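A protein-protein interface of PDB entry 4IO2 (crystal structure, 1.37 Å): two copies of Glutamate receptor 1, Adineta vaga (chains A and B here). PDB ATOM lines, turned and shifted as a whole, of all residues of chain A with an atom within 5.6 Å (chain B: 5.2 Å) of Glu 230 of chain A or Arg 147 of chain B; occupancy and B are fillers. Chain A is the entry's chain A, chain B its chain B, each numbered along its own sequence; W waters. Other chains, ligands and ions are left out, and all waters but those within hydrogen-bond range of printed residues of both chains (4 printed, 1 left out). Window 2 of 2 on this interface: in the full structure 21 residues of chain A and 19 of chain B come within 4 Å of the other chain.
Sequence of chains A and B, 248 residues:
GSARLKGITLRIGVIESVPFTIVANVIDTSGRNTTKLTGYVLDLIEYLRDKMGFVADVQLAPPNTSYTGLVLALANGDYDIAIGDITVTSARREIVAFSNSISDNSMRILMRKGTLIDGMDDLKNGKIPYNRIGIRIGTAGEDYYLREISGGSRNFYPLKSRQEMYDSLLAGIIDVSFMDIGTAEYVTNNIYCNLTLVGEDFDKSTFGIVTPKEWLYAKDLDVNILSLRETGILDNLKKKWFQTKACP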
ATOM      1  N   ILE A 225      33.356 -25.742 -18.622  1.00  0.00           N
ATOM      2  CA  ILE A 225      33.467 -24.646 -19.575  1.00  0.00           C
ATOM      3  C   ILE A 225      32.100 -24.195 -20.063  1.00  0.00           C
ATOM      4  O   ILE A 225      31.828 -22.991 -20.115  1.00  0.00           O
ATOM      5  CB  ILE A 225      34.356 -25.043 -20.790  1.00  0.00           C
ATOM      6  CG1 ILE A 225      35.778 -25.243 -20.344  1.00  0.00           C
ATOM      7  CG2 ILE A 225      34.239 -24.003 -21.926  1.00  0.00           C
ATOM      8  CD1 ILE A 225      36.576 -25.961 -21.395  1.00  0.00           C
ATOM      9  N   LEU A 226      31.237 -25.137 -20.396  1.00  0.00           N
ATOM     10  CA  LEU A 226      29.903 -24.801 -20.931  1.00  0.00           C
ATOM     11  C   LEU A 226      29.069 -24.099 -19.858  1.00  0.00           C
ATOM     12  O   LEU A 226      28.312 -23.216 -20.154  1.00  0.00           O
ATOM     13  CB  LEU A 226      29.242 -26.072 -21.421  1.00  0.00           C
ATOM     14  CG  LEU A 226      29.864 -26.601 -22.719  1.00  0.00           C
ATOM     15  CD1 LEU A 226      29.464 -28.065 -22.969  1.00  0.00           C
ATOM     16  CD2 LEU A 226      29.461 -25.717 -23.886  1.00  0.00           C
ATOM     17  N   SER A 227      29.221 -24.483 -18.602  1.00  0.00           N
ATOM     18  CA  SER A 227      28.543 -23.803 -17.520  1.00  0.00           C
ATOM     19  C   SER A 227      29.044 -22.362 -17.380  1.00  0.00           C
ATOM     20  O   SER A 227      28.230 -21.450 -17.188  1.00  0.00           O
ATOM     21  CB  SER A 227      28.731 -24.563 -16.203  1.00  0.00           C
ATOM     22  OG  SER A 227      28.094 -23.863 -15.170  1.00  0.00           O
ATOM     23  N   LEU A 228      30.359 -22.134 -17.484  1.00  0.00           N
ATOM     24  CA  LEU A 228      30.859 -20.758 -17.470  1.00  0.00           C
ATOM     25  C   LEU A 228      30.320 -19.948 -18.640  1.00  0.00           C
ATOM     26  O   LEU A 228      30.060 -18.743 -18.511  1.00  0.00           O
ATOM     27  CB  LEU A 228      32.391 -20.723 -17.481  1.00  0.00           C
ATOM     28  CG  LEU A 228      33.146 -21.286 -16.269  1.00  0.00           C
ATOM     29  CD1 LEU A 228      34.636 -21.088 -16.429  1.00  0.00           C
ATOM     30  CD2 LEU A 228      32.667 -20.635 -14.954  1.00  0.00           C
ATOM     31  N   ARG A 229      30.162 -20.574 -19.799  1.00  0.00           N
ATOM     32  CA  ARG A 229      29.567 -19.912 -20.947  1.00  0.00           C
ATOM     33  C   ARG A 229      28.114 -19.512 -20.625  1.00  0.00           C
ATOM     34  O   ARG A 229      27.719 -18.327 -20.745  1.00  0.00           O
ATOM     35  CB  ARG A 229      29.658 -20.877 -22.157  1.00  0.00           C
ATOM     36  CG  ARG A 229      29.145 -20.349 -23.531  1.00  0.00           C
ATOM     37  CD  ARG A 229      28.945 -21.490 -24.590  1.00  0.00           C
ATOM     38  NE  ARG A 229      30.209 -22.007 -25.106  1.00  0.00           N
ATOM     39  CZ  ARG A 229      30.334 -22.877 -26.103  1.00  0.00           C
ATOM     40  NH1 ARG A 229      29.279 -23.359 -26.740  1.00  0.00           N
ATOM     41  NH2 ARG A 229      31.539 -23.283 -26.457  1.00  0.00           N
ATOM     42  N   GLU A 230      27.327 -20.485 -20.190  1.00  0.00           N
ATOM     43  CA  GLU A 230      25.894 -20.299 -19.996  1.00  0.00           C
ATOM     44  C   GLU A 230      25.596 -19.247 -18.947  1.00  0.00           C
ATOM     45  O   GLU A 230      24.631 -18.493 -19.096  1.00  0.00           O
ATOM     46  CB  GLU A 230      25.247 -21.647 -19.613  1.00  0.00           C
ATOM     47  CG  GLU A 230      25.191 -22.578 -20.816  1.00  0.00           C
ATOM     48  CD  GLU A 230      25.052 -24.051 -20.500  1.00  0.00           C
ATOM     49  OE1 GLU A 230      24.740 -24.416 -19.367  1.00  0.00           O
ATOM     50  OE2 GLU A 230      25.378 -24.865 -21.395  1.00  0.00           O
ATOM     51  N   THR A 231      26.378 -19.223 -17.869  1.00  0.00           N
ATOM     52  CA  THR A 231      26.179 -18.272 -16.768  1.00  0.00           C
ATOM     53  C   THR A 231      26.803 -16.885 -16.992  1.00  0.00           C
ATOM     54  O   THR A 231      26.708 -16.012 -16.130  1.00  0.00           O
ATOM     55  CB  THR A 231      26.650 -18.887 -15.415  1.00  0.00           C
ATOM     56  OG1 THR A 231      28.080 -19.135 -15.453  1.00  0.00           O
ATOM     57  CG2 THR A 231      25.872 -20.204 -15.127  1.00  0.00           C
ATOM     58  N   GLY A 232      27.398 -16.669 -18.163  1.00  0.00           N
ATOM     59  CA  GLY A 232      27.895 -15.345 -18.515  1.00  0.00           C
ATOM     60  C   GLY A 232      29.311 -15.040 -18.085  1.00  0.00           C
ATOM     61  O   GLY A 232      29.788 -13.933 -18.324  1.00  0.00           O
ATOM     62  N   VAL B  88      25.242 -27.047 -28.261  1.00  0.00           N
ATOM     63  CA  VAL B  88      26.087 -27.680 -27.256  1.00  0.00           C
ATOM     64  C   VAL B  88      25.792 -27.052 -25.901  1.00  0.00           C
ATOM     65  O   VAL B  88      25.952 -25.843 -25.727  1.00  0.00           O
ATOM     66  CB  VAL B  88      27.566 -27.482 -27.614  1.00  0.00           C
ATOM     67  CG1 VAL B  88      28.436 -28.202 -26.648  1.00  0.00           C
ATOM     68  CG2 VAL B  88      27.841 -28.017 -29.032  1.00  0.00           C
ATOM     69  N   THR B  89      25.328 -27.840 -24.956  1.00  0.00           N
ATOM     70  CA  THR B  89      25.008 -27.344 -23.621  1.00  0.00           C
ATOM     71  C   THR B  89      25.666 -28.195 -22.562  1.00  0.00           C
ATOM     72  O   THR B  89      25.974 -29.348 -22.797  1.00  0.00           O
ATOM     73  CB  THR B  89      23.478 -27.328 -23.339  1.00  0.00           C
ATOM     74  OG1 THR B  89      23.026 -28.680 -23.155  1.00  0.00           O
ATOM     75  CG2 THR B  89      22.679 -26.604 -24.407  1.00  0.00           C
ATOM     76  N   SER B  90      25.832 -27.626 -21.374  1.00  0.00           N
ATOM     77  CA  SER B  90      26.446 -28.340 -20.260  1.00  0.00           C
ATOM     78  C   SER B  90      25.648 -29.569 -19.860  1.00  0.00           C
ATOM     79  O   SER B  90      26.217 -30.623 -19.617  1.00  0.00           O
ATOM     80  CB  SER B  90      26.624 -27.429 -19.054  1.00  0.00           C
ATOM     81  OG  SER B  90      25.385 -26.932 -18.531  1.00  0.00           O
ATOM     82  N   ALA B  91      24.335 -29.441 -19.802  1.00  0.00           N
ATOM     83  CA  ALA B  91      23.504 -30.591 -19.393  1.00  0.00           C
ATOM     84  C   ALA B  91      23.549 -31.691 -20.432  1.00  0.00           C
ATOM     85  O   ALA B  91      23.515 -32.895 -20.099  1.00  0.00           O
ATOM     86  CB  ALA B  91      22.061 -30.142 -19.149  1.00  0.00           C
ATOM     87  N   GLU B 142      14.805 -22.869 -23.499  1.00  0.00           N
ATOM     88  CA  GLU B 142      14.166 -23.131 -22.211  1.00  0.00           C
ATOM     89  C   GLU B 142      15.143 -22.890 -21.061  1.00  0.00           C
ATOM     90  O   GLU B 142      14.799 -22.319 -20.003  1.00  0.00           O
ATOM     91  CB  GLU B 142      13.673 -24.578 -22.141  1.00  0.00           C
ATOM     92  CG  GLU B 142      12.937 -24.932 -20.870  1.00  0.00           C
ATOM     93  CD  GLU B 142      12.566 -26.381 -20.823  1.00  0.00           C
ATOM     94  OE1 GLU B 142      13.147 -27.217 -21.599  1.00  0.00           O
ATOM     95  OE2 GLU B 142      11.704 -26.702 -19.998  1.00  0.00           O
ATOM     96  N   ASP B 143      16.369 -23.342 -21.254  1.00  0.00           N
ATOM     97  CA  ASP B 143      17.377 -23.128 -20.247  1.00  0.00           C
ATOM     98  C   ASP B 143      17.658 -21.685 -19.983  1.00  0.00           C
ATOM     99  O   ASP B 143      17.805 -21.261 -18.798  1.00  0.00           O
ATOM    100  CB  ASP B 143      18.687 -23.765 -20.744  1.00  0.00           C
ATOM    101  CG  ASP B 143      19.503 -24.384 -19.644  1.00  0.00           C
ATOM    102  OD1 ASP B 143      19.208 -24.141 -18.462  1.00  0.00           O
ATOM    103  OD2 ASP B 143      20.440 -25.158 -19.978  1.00  0.00           O
ATOM    104  N   TYR B 144      17.738 -20.912 -21.066  1.00  0.00           N
ATOM    105  CA  TYR B 144      17.995 -19.492 -20.958  1.00  0.00           C
ATOM    106  C   TYR B 144      16.840 -18.854 -20.193  1.00  0.00           C
ATOM    107  O   TYR B 144      17.058 -18.062 -19.287  1.00  0.00           O
ATOM    108  CB  TYR B 144      18.183 -18.824 -22.349  1.00  0.00           C
ATOM    109  CG  TYR B 144      18.370 -17.312 -22.265  1.00  0.00           C
ATOM    110  CD1 TYR B 144      17.277 -16.457 -22.246  1.00  0.00           C
ATOM    111  CD2 TYR B 144      19.642 -16.734 -22.192  1.00  0.00           C
ATOM    112  CE1 TYR B 144      17.422 -15.086 -22.141  1.00  0.00           C
ATOM    113  CE2 TYR B 144      19.791 -15.330 -22.088  1.00  0.00           C
ATOM    114  CZ  TYR B 144      18.676 -14.521 -22.074  1.00  0.00           C
ATOM    115  OH  TYR B 144      18.792 -13.129 -21.963  1.00  0.00           O
ATOM    116  N   TYR B 145      15.618 -19.224 -20.534  1.00  0.00           N
ATOM    117  CA  TYR B 145      14.421 -18.686 -19.869  1.00  0.00           C
ATOM    118  C   TYR B 145      14.487 -18.926 -18.371  1.00  0.00           C
ATOM    119  O   TYR B 145      14.252 -18.003 -17.559  1.00  0.00           O
ATOM    120  CB  TYR B 145      13.143 -19.298 -20.466  1.00  0.00           C
ATOM    121  CG  TYR B 145      11.881 -18.744 -19.856  1.00  0.00           C
ATOM    122  CD1 TYR B 145      11.354 -19.281 -18.677  1.00  0.00           C
ATOM    123  CD2 TYR B 145      11.245 -17.643 -20.398  1.00  0.00           C
ATOM    124  CE1 TYR B 145      10.174 -18.794 -18.120  1.00  0.00           C
ATOM    125  CE2 TYR B 145      10.090 -17.144 -19.813  1.00  0.00           C
ATOM    126  CZ  TYR B 145       9.594 -17.705 -18.678  1.00  0.00           C
ATOM    127  OH  TYR B 145       8.465 -17.192 -18.127  1.00  0.00           O
ATOM    128  N   LEU B 146      14.729 -20.173 -17.973  1.00  0.00           N
ATOM    129  CA  LEU B 146      14.732 -20.504 -16.559  1.00  0.00           C
ATOM    130  C   LEU B 146      15.856 -19.775 -15.817  1.00  0.00           C
ATOM    131  O   LEU B 146      15.639 -19.346 -14.669  1.00  0.00           O
ATOM    132  CB  LEU B 146      14.853 -22.028 -16.390  1.00  0.00           C
ATOM    133  CG  LEU B 146      13.644 -22.828 -16.886  1.00  0.00           C
ATOM    134  CD1 LEU B 146      13.928 -24.357 -16.943  1.00  0.00           C
ATOM    135  CD2 LEU B 146      12.426 -22.511 -16.029  1.00  0.00           C
ATOM    136  N   ARG B 147      17.007 -19.576 -16.436  1.00  0.00           N
ATOM    137  CA  ARG B 147      18.106 -18.890 -15.736  1.00  0.00           C
ATOM    138  C   ARG B 147      18.007 -17.356 -15.704  1.00  0.00           C
ATOM    139  O   ARG B 147      18.477 -16.703 -14.766  1.00  0.00           O
ATOM    140  CB  ARG B 147      19.414 -19.267 -16.409  1.00  0.00           C
ATOM    141  CG  ARG B 147      20.643 -18.889 -15.655  1.00  0.00           C
ATOM    142  CD  ARG B 147      21.847 -18.911 -16.609  1.00  0.00           C
ATOM    143  NE  ARG B 147      21.662 -19.804 -17.764  1.00  0.00           N
ATOM    144  CZ  ARG B 147      21.674 -19.420 -19.035  1.00  0.00           C
ATOM    145  NH1 ARG B 147      21.877 -18.156 -19.371  1.00  0.00           N
ATOM    146  NH2 ARG B 147      21.488 -20.319 -19.997  1.00  0.00           N
ATOM    147  N   GLU B 148      17.454 -16.774 -16.754  1.00  0.00           N
ATOM    148  CA  GLU B 148      17.520 -15.325 -16.916  1.00  0.00           C
ATOM    149  C   GLU B 148      16.214 -14.580 -16.764  1.00  0.00           C
ATOM    150  O   GLU B 148      16.243 -13.387 -16.486  1.00  0.00           O
ATOM    151  CB  GLU B 148      18.121 -15.015 -18.311  1.00  0.00           C
ATOM    152  CG  GLU B 148      19.430 -15.690 -18.587  1.00  0.00           C
ATOM    153  CD  GLU B 148      20.557 -15.188 -17.777  1.00  0.00           C
ATOM    154  OE1 GLU B 148      20.467 -14.096 -17.216  1.00  0.00           O
ATOM    155  OE2 GLU B 148      21.596 -15.893 -17.746  1.00  0.00           O
ATOM    156  N   ILE B 149      15.102 -15.249 -17.017  1.00  0.00           N
ATOM    157  CA  ILE B 149      13.794 -14.610 -16.962  1.00  0.00           C
ATOM    158  C   ILE B 149      13.010 -14.947 -15.702  1.00  0.00           C
ATOM    159  O   ILE B 149      12.524 -14.054 -15.008  1.00  0.00           O
ATOM    160  CB  ILE B 149      12.932 -14.968 -18.194  1.00  0.00           C
ATOM    161  CG1 ILE B 149      13.635 -14.639 -19.520  1.00  0.00           C
ATOM    162  CG2 ILE B 149      11.571 -14.295 -18.093  1.00  0.00           C
ATOM    163  CD1 ILE B 149      14.132 -13.242 -19.604  1.00  0.00           C
ATOM    164  N   GLY B 151      13.749 -17.015 -12.827  1.00  0.00           N
ATOM    165  CA  GLY B 151      14.319 -17.391 -11.555  1.00  0.00           C
ATOM    166  C   GLY B 151      14.103 -18.861 -11.280  1.00  0.00           C
ATOM    167  O   GLY B 151      13.925 -19.285 -10.145  1.00  0.00           O
ATOM    168  N   GLY B 152      14.078 -19.650 -12.336  1.00  0.00           N
ATOM    169  CA  GLY B 152      13.973 -21.085 -12.202  1.00  0.00           C
ATOM    170  C   GLY B 152      12.562 -21.639 -12.255  1.00  0.00           C
ATOM    171  O   GLY B 152      12.378 -22.850 -12.221  1.00  0.00           O
ATOM    172  N   ASP B 203      22.578 -15.397 -25.826  1.00  0.00           N
ATOM    173  CA  ASP B 203      22.966 -16.786 -25.636  1.00  0.00           C
ATOM    174  C   ASP B 203      23.900 -17.267 -26.748  1.00  0.00           C
ATOM    175  O   ASP B 203      23.645 -18.296 -27.395  1.00  0.00           O
ATOM    176  CB  ASP B 203      21.753 -17.701 -25.523  1.00  0.00           C
ATOM    177  CG  ASP B 203      22.064 -18.979 -24.746  1.00  0.00           C
ATOM    178  OD1 ASP B 203      22.873 -18.920 -23.787  1.00  0.00           O
ATOM    179  OD2 ASP B 203      21.534 -20.061 -25.117  1.00  0.00           O
HETATM  180  O   HOH W   1      23.244 -17.242 -21.856  1.00  0.00           O
HETATM  181  O   HOH W   2      22.875 -26.755 -19.780  1.00  0.00           O
HETATM  182  O   HOH W   3      26.895 -23.637 -26.972  1.00  0.00           O
HETATM  183  O   HOH W   4      25.367 -23.688 -24.010  1.00  0.00           O
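The backbone carbonyl oxygen of Ser 227 of chain A is in hydrogen-bond range of the side-chain hydroxyl of Thr 231 of chain A.
NH1 of Arg 147 of chain B is in salt-bridge range of OE2 of Glu 148 of chain B, 2.8 Å away.
The side-chain carboxylate of Glu 230 of chain A lies within hydrogen-bond range of the side-chain hydroxyl of Ser 90 of chain B, at 2.7 Å.
The guanidinium group (NH1) of Arg 147 of chain B lies within hydrogen-bond range of the backbone carbonyl oxygen (O) of Glu 230 of chain A, at 2.8 Å.
Of the 8 printed residues of chain A, 3 touch a printed residue of chain B.
Along chain A the printed residues that touch a printed residue of chain B span positions 226 to 230.
Hydrophobic or aromatic side chains of chain B within 4 Å of the printed part of chain A: Val 88.
Among the printed residues, no Asp or Glu carboxylate lies within 4 Å of a Lys or Arg side-chain nitrogen of the other chain.
No position is printed for both chains.
Val 88 of chain B touches Leu 226 of chain A (CG1 to CD1, 3.8 Å).
CD1 of Leu 226 of chain A touches O of Thr 89 of chain B (3.7 Å).
Ser 90 of chain B touches Leu 226 of chain A (N to CB, 3.7 Å).
Ser 227 of chain A touches Ser 90 of chain B (N to CB, 3.95 Å).
Thr 89 of chain B touches Glu 230 of chain A.
Printed residues of chain B within 4 Å of Glu 230 of chain A: Thr 89, Ser 90 and Arg 147.
Of the printed residues of chain A, Arg 147 of chain B touches Glu 230 (2.8 Å).
Of the printed residues of chain A, Val 88 of chain B touches Leu 226.
Of the printed residues of chain B, Leu 226 of chain A touches Val 88 (3.8 Å), Thr 89 (3.7 Å) and Ser 90 (3.7 Å).
Of the printed residues of chain B, Ser 227 of chain A touches Ser 90.
Printed residues of chain A within 4 Å of Ser 90 of chain B: Leu 226, Ser 227 and Glu 230.
Of the printed residues of chain A, Thr 89 of chain B touches Leu 226 (3.7 Å) and Glu 230 (3.4 Å).
Tyr 145 of chain B touches none of the printed residues of chain A.
Ala 91 of chain B touches none of the printed residues of chain A.
Water W3 lies within hydrogen-bond range of the guanidinium group of Arg 229 of chain A (2.4 Å) and the backbone carbonyl oxygen of Val 88 of chain B (2.7 Å).
Water W1 lies within hydrogen-bond range of OD1 of Asp 203 of chain B (2.6 Å), NH1 of Arg 147 of chain B (3.0 Å) and O of Glu 230 of chain A (3.3 Å).
Water W2 lies within hydrogen-bond range of the side-chain hydroxyl (OG) of Ser 90 of chain B (2.8 Å), the side-chain carboxylate (OD2) of Asp 143 of chain B (2.9 Å), the side-chain carboxylate (OE1) of Glu 230 of chain A (3.0 Å) and the backbone NH (N) of Ala 91 of chain B (3.1 Å).
Water W4 lies within hydrogen-bond range of O of Val 88 of chain B and OE2 of Glu 230 of chain A.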
